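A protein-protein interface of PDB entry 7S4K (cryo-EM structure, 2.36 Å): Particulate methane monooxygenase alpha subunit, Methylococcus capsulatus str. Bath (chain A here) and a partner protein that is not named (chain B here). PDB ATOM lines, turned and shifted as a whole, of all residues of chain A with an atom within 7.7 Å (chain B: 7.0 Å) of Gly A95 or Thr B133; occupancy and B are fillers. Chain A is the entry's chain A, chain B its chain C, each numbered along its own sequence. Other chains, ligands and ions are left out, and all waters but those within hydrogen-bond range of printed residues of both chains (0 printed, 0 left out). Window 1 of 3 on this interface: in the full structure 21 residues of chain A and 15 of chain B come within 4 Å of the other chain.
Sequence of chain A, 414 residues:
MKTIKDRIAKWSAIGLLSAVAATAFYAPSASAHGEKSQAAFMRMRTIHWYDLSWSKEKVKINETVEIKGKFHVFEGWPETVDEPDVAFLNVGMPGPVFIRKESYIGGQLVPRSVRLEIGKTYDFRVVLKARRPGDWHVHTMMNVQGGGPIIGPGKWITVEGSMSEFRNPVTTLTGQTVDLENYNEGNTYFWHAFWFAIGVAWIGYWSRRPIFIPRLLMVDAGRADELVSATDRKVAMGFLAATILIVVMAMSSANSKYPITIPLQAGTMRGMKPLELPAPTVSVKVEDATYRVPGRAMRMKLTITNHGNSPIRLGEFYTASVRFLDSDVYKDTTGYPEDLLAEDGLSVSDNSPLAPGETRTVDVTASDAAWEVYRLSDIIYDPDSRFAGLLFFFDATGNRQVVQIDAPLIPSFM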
ATOM      1  N   VAL A  91     -34.809 -14.574 -20.870  1.00  0.00           N
ATOM      2  CA  VAL A  91     -33.905 -13.754 -20.078  1.00  0.00           C
ATOM      3  C   VAL A  91     -32.588 -13.645 -20.828  1.00  0.00           C
ATOM      4  O   VAL A  91     -32.008 -14.662 -21.222  1.00  0.00           O
ATOM      5  CB  VAL A  91     -33.676 -14.339 -18.672  1.00  0.00           C
ATOM      6  CG1 VAL A  91     -32.864 -13.378 -17.835  1.00  0.00           C
ATOM      7  CG2 VAL A  91     -34.998 -14.635 -18.002  1.00  0.00           C
ATOM      8  N   GLY A  92     -32.122 -12.418 -21.032  1.00  0.00           N
ATOM      9  CA  GLY A  92     -30.836 -12.203 -21.660  1.00  0.00           C
ATOM     10  C   GLY A  92     -29.709 -12.233 -20.653  1.00  0.00           C
ATOM     11  O   GLY A  92     -29.562 -11.305 -19.855  1.00  0.00           O
ATOM     12  N   MET A  93     -28.914 -13.295 -20.667  1.00  0.00           N
ATOM     13  CA  MET A  93     -27.834 -13.459 -19.707  1.00  0.00           C
ATOM     14  C   MET A  93     -26.757 -14.323 -20.341  1.00  0.00           C
ATOM     15  O   MET A  93     -27.039 -15.090 -21.268  1.00  0.00           O
ATOM     16  CB  MET A  93     -28.347 -14.093 -18.408  1.00  0.00           C
ATOM     17  CG  MET A  93     -29.041 -15.424 -18.604  1.00  0.00           C
ATOM     18  SD  MET A  93     -29.709 -16.070 -17.067  1.00  0.00           S
ATOM     19  CE  MET A  93     -29.799 -14.562 -16.117  1.00  0.00           C
ATOM     20  N   PRO A  94     -25.510 -14.220 -19.871  1.00  0.00           N
ATOM     21  CA  PRO A  94     -24.440 -15.041 -20.453  1.00  0.00           C
ATOM     22  C   PRO A  94     -24.486 -16.478 -19.965  1.00  0.00           C
ATOM     23  O   PRO A  94     -23.665 -16.883 -19.138  1.00  0.00           O
ATOM     24  CB  PRO A  94     -23.157 -14.339 -19.987  1.00  0.00           C
ATOM     25  CG  PRO A  94     -23.595 -13.097 -19.267  1.00  0.00           C
ATOM     26  CD  PRO A  94     -24.998 -13.312 -18.837  1.00  0.00           C
ATOM     27  N   GLY A  95     -25.435 -17.258 -20.469  1.00  0.00           N
ATOM     28  CA  GLY A  95     -25.608 -18.616 -20.019  1.00  0.00           C
ATOM     29  C   GLY A  95     -26.307 -18.670 -18.678  1.00  0.00           C
ATOM     30  O   GLY A  95     -26.806 -17.662 -18.173  1.00  0.00           O
ATOM     31  N   PRO A  96     -26.348 -19.846 -18.069  1.00  0.00           N
ATOM     32  CA  PRO A  96     -27.084 -20.019 -16.803  1.00  0.00           C
ATOM     33  C   PRO A  96     -26.308 -19.511 -15.589  1.00  0.00           C
ATOM     34  O   PRO A  96     -26.037 -20.248 -14.640  1.00  0.00           O
ATOM     35  CB  PRO A  96     -27.310 -21.536 -16.755  1.00  0.00           C
ATOM     36  CG  PRO A  96     -26.694 -22.109 -18.002  1.00  0.00           C
ATOM     37  CD  PRO A  96     -25.751 -21.104 -18.530  1.00  0.00           C
ATOM     38  N   VAL A  97     -25.940 -18.228 -15.616  1.00  0.00           N
ATOM     39  CA  VAL A  97     -25.433 -17.591 -14.407  1.00  0.00           C
ATOM     40  C   VAL A  97     -26.547 -17.410 -13.387  1.00  0.00           C
ATOM     41  O   VAL A  97     -26.276 -17.292 -12.188  1.00  0.00           O
ATOM     42  CB  VAL A  97     -24.764 -16.248 -14.738  1.00  0.00           C
ATOM     43  CG1 VAL A  97     -23.605 -16.471 -15.684  1.00  0.00           C
ATOM     44  CG2 VAL A  97     -25.764 -15.285 -15.343  1.00  0.00           C
ATOM     45  N   PHE A  98     -27.793 -17.384 -13.849  1.00  0.00           N
ATOM     46  CA  PHE A  98     -28.985 -17.508 -13.028  1.00  0.00           C
ATOM     47  C   PHE A  98     -29.792 -18.650 -13.614  1.00  0.00           C
ATOM     48  O   PHE A  98     -29.657 -18.952 -14.803  1.00  0.00           O
ATOM     49  CB  PHE A  98     -29.831 -16.232 -13.053  1.00  0.00           C
ATOM     50  CG  PHE A  98     -29.229 -15.073 -12.326  1.00  0.00           C
ATOM     51  CD1 PHE A  98     -29.475 -14.875 -10.984  1.00  0.00           C
ATOM     52  CD2 PHE A  98     -28.427 -14.166 -12.992  1.00  0.00           C
ATOM     53  CE1 PHE A  98     -28.931 -13.802 -10.322  1.00  0.00           C
ATOM     54  CE2 PHE A  98     -27.882 -13.094 -12.334  1.00  0.00           C
ATOM     55  CZ  PHE A  98     -28.136 -12.911 -10.998  1.00  0.00           C
ATOM     56  N   ILE A  99     -30.624 -19.281 -12.806  1.00  0.00           N
ATOM     57  CA  ILE A  99     -31.629 -20.193 -13.332  1.00  0.00           C
ATOM     58  C   ILE A  99     -32.987 -19.518 -13.233  1.00  0.00           C
ATOM     59  O   ILE A  99     -33.316 -18.902 -12.213  1.00  0.00           O
ATOM     60  CB  ILE A  99     -31.612 -21.542 -12.593  1.00  0.00           C
ATOM     61  CG1 ILE A  99     -31.807 -21.358 -11.093  1.00  0.00           C
ATOM     62  CG2 ILE A  99     -30.321 -22.285 -12.882  1.00  0.00           C
ATOM     63  CD1 ILE A  99     -32.592 -22.471 -10.457  1.00  0.00           C
ATOM     64  N   ARG A 131     -26.636 -18.436  -9.515  1.00  0.00           N
ATOM     65  CA  ARG A 131     -25.926 -19.697  -9.690  1.00  0.00           C
ATOM     66  C   ARG A 131     -24.424 -19.528  -9.848  1.00  0.00           C
ATOM     67  O   ARG A 131     -23.666 -20.344  -9.325  1.00  0.00           O
ATOM     68  CB  ARG A 131     -26.493 -20.438 -10.905  1.00  0.00           C
ATOM     69  CG  ARG A 131     -25.899 -21.809 -11.136  1.00  0.00           C
ATOM     70  CD  ARG A 131     -26.635 -22.525 -12.241  1.00  0.00           C
ATOM     71  NE  ARG A 131     -25.981 -23.767 -12.631  1.00  0.00           N
ATOM     72  CZ  ARG A 131     -25.261 -23.916 -13.734  1.00  0.00           C
ATOM     73  NH1 ARG A 131     -25.057 -22.910 -14.566  1.00  0.00           N
ATOM     74  NH2 ARG A 131     -24.735 -25.105 -14.008  1.00  0.00           N
ATOM     75  N   ARG A 132     -23.975 -18.487 -10.541  1.00  0.00           N
ATOM     76  CA  ARG A 132     -22.568 -18.311 -10.843  1.00  0.00           C
ATOM     77  C   ARG A 132     -22.098 -16.942 -10.376  1.00  0.00           C
ATOM     78  O   ARG A 132     -22.707 -15.927 -10.739  1.00  0.00           O
ATOM     79  CB  ARG A 132     -22.314 -18.459 -12.343  1.00  0.00           C
ATOM     80  CG  ARG A 132     -21.882 -19.843 -12.759  1.00  0.00           C
ATOM     81  CD  ARG A 132     -21.512 -19.873 -14.222  1.00  0.00           C
ATOM     82  NE  ARG A 132     -20.224 -19.236 -14.463  1.00  0.00           N
ATOM     83  CZ  ARG A 132     -19.908 -18.588 -15.575  1.00  0.00           C
ATOM     84  NH1 ARG A 132     -20.762 -18.478 -16.576  1.00  0.00           N
ATOM     85  NH2 ARG A 132     -18.703 -18.038 -15.684  1.00  0.00           N
ATOM     86  N   TRP A 136     -23.154  -9.771 -13.943  1.00  0.00           N
ATOM     87  CA  TRP A 136     -23.916 -10.211 -15.098  1.00  0.00           C
ATOM     88  C   TRP A 136     -24.913  -9.145 -15.519  1.00  0.00           C
ATOM     89  O   TRP A 136     -25.625  -8.571 -14.692  1.00  0.00           O
ATOM     90  CB  TRP A 136     -24.642 -11.524 -14.806  1.00  0.00           C
ATOM     91  CG  TRP A 136     -23.765 -12.532 -14.147  1.00  0.00           C
ATOM     92  CD1 TRP A 136     -23.884 -13.021 -12.885  1.00  0.00           C
ATOM     93  CD2 TRP A 136     -22.616 -13.161 -14.716  1.00  0.00           C
ATOM     94  NE1 TRP A 136     -22.888 -13.925 -12.633  1.00  0.00           N
ATOM     95  CE2 TRP A 136     -22.093 -14.028 -13.743  1.00  0.00           C
ATOM     96  CE3 TRP A 136     -21.982 -13.080 -15.957  1.00  0.00           C
ATOM     97  CZ2 TRP A 136     -20.967 -14.809 -13.971  1.00  0.00           C
ATOM     98  CZ3 TRP A 136     -20.867 -13.854 -16.181  1.00  0.00           C
ATOM     99  CH2 TRP A 136     -20.370 -14.707 -15.194  1.00  0.00           C
ATOM    100  N   MET A 141     -35.967 -10.197 -22.187  1.00  0.00           N
ATOM    101  CA  MET A 141     -36.153 -10.236 -23.624  1.00  0.00           C
ATOM    102  C   MET A 141     -37.398 -11.032 -23.992  1.00  0.00           C
ATOM    103  O   MET A 141     -37.932 -11.813 -23.206  1.00  0.00           O
ATOM    104  CB  MET A 141     -34.923 -10.833 -24.298  1.00  0.00           C
ATOM    105  CG  MET A 141     -34.484 -12.134 -23.685  1.00  0.00           C
ATOM    106  SD  MET A 141     -33.057 -12.840 -24.511  1.00  0.00           S
ATOM    107  CE  MET A 141     -33.415 -12.416 -26.203  1.00  0.00           C
ATOM    108  N   TRP B  45     -16.574 -13.850 -22.117  1.00  0.00           N
ATOM    109  CA  TRP B  45     -17.152 -12.724 -21.409  1.00  0.00           C
ATOM    110  C   TRP B  45     -16.028 -11.779 -21.016  1.00  0.00           C
ATOM    111  O   TRP B  45     -14.850 -12.092 -21.205  1.00  0.00           O
ATOM    112  CB  TRP B  45     -17.919 -13.187 -20.169  1.00  0.00           C
ATOM    113  CG  TRP B  45     -18.448 -14.585 -20.262  1.00  0.00           C
ATOM    114  CD1 TRP B  45     -19.741 -14.960 -20.481  1.00  0.00           C
ATOM    115  CD2 TRP B  45     -17.700 -15.796 -20.120  1.00  0.00           C
ATOM    116  NE1 TRP B  45     -19.842 -16.328 -20.496  1.00  0.00           N
ATOM    117  CE2 TRP B  45     -18.601 -16.865 -20.276  1.00  0.00           C
ATOM    118  CE3 TRP B  45     -16.352 -16.080 -19.884  1.00  0.00           C
ATOM    119  CZ2 TRP B  45     -18.201 -18.192 -20.202  1.00  0.00           C
ATOM    120  CZ3 TRP B  45     -15.958 -17.396 -19.811  1.00  0.00           C
ATOM    121  CH2 TRP B  45     -16.877 -18.436 -19.968  1.00  0.00           C
ATOM    122  N   ASP B 127     -18.935 -23.204 -31.646  1.00  0.00           N
ATOM    123  CA  ASP B 127     -19.699 -22.069 -32.219  1.00  0.00           C
ATOM    124  C   ASP B 127     -21.168 -22.294 -31.889  1.00  0.00           C
ATOM    125  O   ASP B 127     -21.835 -21.317 -31.506  1.00  0.00           O
ATOM    126  CB  ASP B 127     -19.486 -21.984 -33.726  1.00  0.00           C
ATOM    127  CG  ASP B 127     -19.983 -20.702 -34.361  1.00  0.00           C
ATOM    128  OD1 ASP B 127     -19.429 -19.640 -34.036  1.00  0.00           O
ATOM    129  OD2 ASP B 127     -20.885 -20.812 -35.273  1.00  0.00           O
ATOM    130  N   GLY B 128     -21.605 -23.557 -31.909  1.00  0.00           N
ATOM    131  CA  GLY B 128     -22.984 -23.899 -31.514  1.00  0.00           C
ATOM    132  C   GLY B 128     -23.273 -23.524 -30.073  1.00  0.00           C
ATOM    133  O   GLY B 128     -24.308 -22.899 -29.868  1.00  0.00           O
ATOM    134  N   THR B 129     -22.398 -23.876 -29.118  1.00  0.00           N
ATOM    135  CA  THR B 129     -22.607 -23.433 -27.708  1.00  0.00           C
ATOM    136  C   THR B 129     -22.908 -21.931 -27.714  1.00  0.00           C
ATOM    137  O   THR B 129     -23.988 -21.555 -27.241  1.00  0.00           O
ATOM    138  CB  THR B 129     -21.437 -23.786 -26.768  1.00  0.00           C
ATOM    139  OG1 THR B 129     -20.507 -22.707 -26.657  1.00  0.00           O
ATOM    140  CG2 THR B 129     -20.672 -25.021 -27.188  1.00  0.00           C
ATOM    141  N   TRP B 130     -22.016 -21.127 -28.296  1.00  0.00           N
ATOM    142  CA  TRP B 130     -22.203 -19.653 -28.344  1.00  0.00           C
ATOM    143  C   TRP B 130     -23.491 -19.298 -29.097  1.00  0.00           C
ATOM    144  O   TRP B 130     -24.138 -18.314 -28.695  1.00  0.00           O
ATOM    145  CB  TRP B 130     -20.964 -19.003 -28.975  1.00  0.00           C
ATOM    146  CG  TRP B 130     -20.357 -17.866 -28.208  1.00  0.00           C
ATOM    147  CD1 TRP B 130     -19.961 -16.668 -28.729  1.00  0.00           C
ATOM    148  CD2 TRP B 130     -20.039 -17.812 -26.802  1.00  0.00           C
ATOM    149  NE1 TRP B 130     -19.434 -15.870 -27.751  1.00  0.00           N
ATOM    150  CE2 TRP B 130     -19.467 -16.544 -26.559  1.00  0.00           C
ATOM    151  CE3 TRP B 130     -20.178 -18.695 -25.724  1.00  0.00           C
ATOM    152  CZ2 TRP B 130     -19.045 -16.144 -25.292  1.00  0.00           C
ATOM    153  CZ3 TRP B 130     -19.761 -18.300 -24.472  1.00  0.00           C
ATOM    154  CH2 TRP B 130     -19.201 -17.040 -24.261  1.00  0.00           C
ATOM    155  N   HIS B 131     -23.871 -20.075 -30.124  1.00  0.00           N
ATOM    156  CA  HIS B 131     -25.059 -19.728 -30.964  1.00  0.00           C
ATOM    157  C   HIS B 131     -26.310 -20.354 -30.330  1.00  0.00           C
ATOM    158  O   HIS B 131     -27.215 -20.723 -31.092  1.00  0.00           O
ATOM    159  CB  HIS B 131     -24.755 -19.963 -32.474  1.00  0.00           C
ATOM    160  CG  HIS B 131     -23.692 -18.998 -32.889  1.00  0.00           C
ATOM    161  ND1 HIS B 131     -23.324 -18.035 -31.964  1.00  0.00           N
ATOM    162  CD2 HIS B 131     -22.815 -18.879 -33.880  1.00  0.00           C
ATOM    163  CE1 HIS B 131     -22.359 -17.304 -32.388  1.00  0.00           C
ATOM    164  NE2 HIS B 131     -22.037 -17.812 -33.507  1.00  0.00           N
ATOM    165  N   GLN B 132     -26.332 -20.493 -28.997  1.00  0.00           N
ATOM    166  CA  GLN B 132     -27.520 -20.982 -28.242  1.00  0.00           C
ATOM    167  C   GLN B 132     -27.499 -20.298 -26.869  1.00  0.00           C
ATOM    168  O   GLN B 132     -28.544 -20.333 -26.194  1.00  0.00           O
ATOM    169  CB  GLN B 132     -27.515 -22.489 -27.962  1.00  0.00           C
ATOM    170  CG  GLN B 132     -27.210 -23.418 -29.132  1.00  0.00           C
ATOM    171  CD  GLN B 132     -28.360 -23.759 -30.046  1.00  0.00           C
ATOM    172  OE1 GLN B 132     -28.275 -23.603 -31.261  1.00  0.00           O
ATOM    173  NE2 GLN B 132     -29.435 -24.271 -29.474  1.00  0.00           N
ATOM    174  N   THR B 133     -26.368 -19.694 -26.475  1.00  0.00           N
ATOM    175  CA  THR B 133     -26.228 -19.112 -25.109  1.00  0.00           C
ATOM    176  C   THR B 133     -26.304 -17.584 -25.096  1.00  0.00           C
ATOM    177  O   THR B 133     -26.684 -17.050 -24.042  1.00  0.00           O
ATOM    178  CB  THR B 133     -24.874 -19.457 -24.478  1.00  0.00           C
ATOM    179  OG1 THR B 133     -23.824 -18.955 -25.308  1.00  0.00           O
ATOM    180  CG2 THR B 133     -24.685 -20.940 -24.276  1.00  0.00           C
ATOM    181  N   ILE B 134     -25.860 -16.913 -26.164  1.00  0.00           N
ATOM    182  CA  ILE B 134     -25.827 -15.418 -26.175  1.00  0.00           C
ATOM    183  C   ILE B 134     -26.482 -14.902 -27.462  1.00  0.00           C
ATOM    184  O   ILE B 134     -26.475 -15.643 -28.465  1.00  0.00           O
ATOM    185  CB  ILE B 134     -24.390 -14.872 -26.013  1.00  0.00           C
ATOM    186  CG1 ILE B 134     -23.408 -15.503 -27.004  1.00  0.00           C
ATOM    187  CG2 ILE B 134     -23.903 -15.010 -24.576  1.00  0.00           C
ATOM    188  CD1 ILE B 134     -22.903 -14.546 -28.059  1.00  0.00           C
ATOM    189  N   VAL B 135     -27.010 -13.674 -27.430  1.00  0.00           N
ATOM    190  CA  VAL B 135     -27.636 -13.062 -28.642  1.00  0.00           C
ATOM    191  C   VAL B 135     -26.528 -12.673 -29.627  1.00  0.00           C
ATOM    192  O   VAL B 135     -25.589 -11.968 -29.204  1.00  0.00           O
ATOM    193  CB  VAL B 135     -28.518 -11.853 -28.272  1.00  0.00           C
ATOM    194  CG1 VAL B 135     -29.120 -11.182 -29.494  1.00  0.00           C
ATOM    195  CG2 VAL B 135     -29.614 -12.226 -27.292  1.00  0.00           C
ATOM    196  N   GLU B 209     -31.952 -19.262 -33.750  1.00  0.00           N
ATOM    197  CA  GLU B 209     -30.625 -19.873 -33.623  1.00  0.00           C
ATOM    198  C   GLU B 209     -30.656 -21.369 -33.908  1.00  0.00           C
ATOM    199  O   GLU B 209     -29.860 -22.105 -33.318  1.00  0.00           O
ATOM    200  CB  GLU B 209     -30.044 -19.617 -32.230  1.00  0.00           C
ATOM    201  CG  GLU B 209     -29.297 -18.299 -32.092  1.00  0.00           C
ATOM    202  CD  GLU B 209     -28.253 -18.073 -33.173  1.00  0.00           C
ATOM    203  OE1 GLU B 209     -27.695 -19.057 -33.703  1.00  0.00           O
ATOM    204  OE2 GLU B 209     -27.987 -16.897 -33.495  1.00  0.00           O
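The backbone carbonyl oxygen of Met A93 sits close to the backbone carbonyl oxygen of Thr B133, 3.4 Å away.
N of Gly A92 sits close to SD of Met A141 (3.6 Å).
The backbone carbonyl oxygen (O) of Thr B129 sits close to the side-chain hydroxyl (OG1) of Thr B133, 3.2 Å away.
The backbone carbonyl oxygen of Trp B130 sits at hydrogen-bond distance from the side-chain hydroxyl of Thr B133 (3.5 Å).
Among the printed residues, merely in contact across the chains: Pro A94 with Trp B45 (3.5 Å), Gly A95 with Thr B133 (3.8 Å) and Met A141 with Val B135 (3.96 Å).
Of chain B, only Thr B133 comes within 4 Å of Gly A95.
Thr B133 touches two residues of chain A.
Printed residues of chain B within 4 Å of Met A93: Thr B133 (3.4 Å).
Printed residues of chain A within 4 Å of Trp B45: Pro A94 (3.5 Å).
Trp A136 touches none of the printed residues of chain B.
Trp B130 touches none of the printed residues of chain A.
Hydrophobic or aromatic side chains of chain B within 4 Å of the printed part of chain A: Trp B45 and Val B135.
Among the printed residues, 4 pairs touch across the chains.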
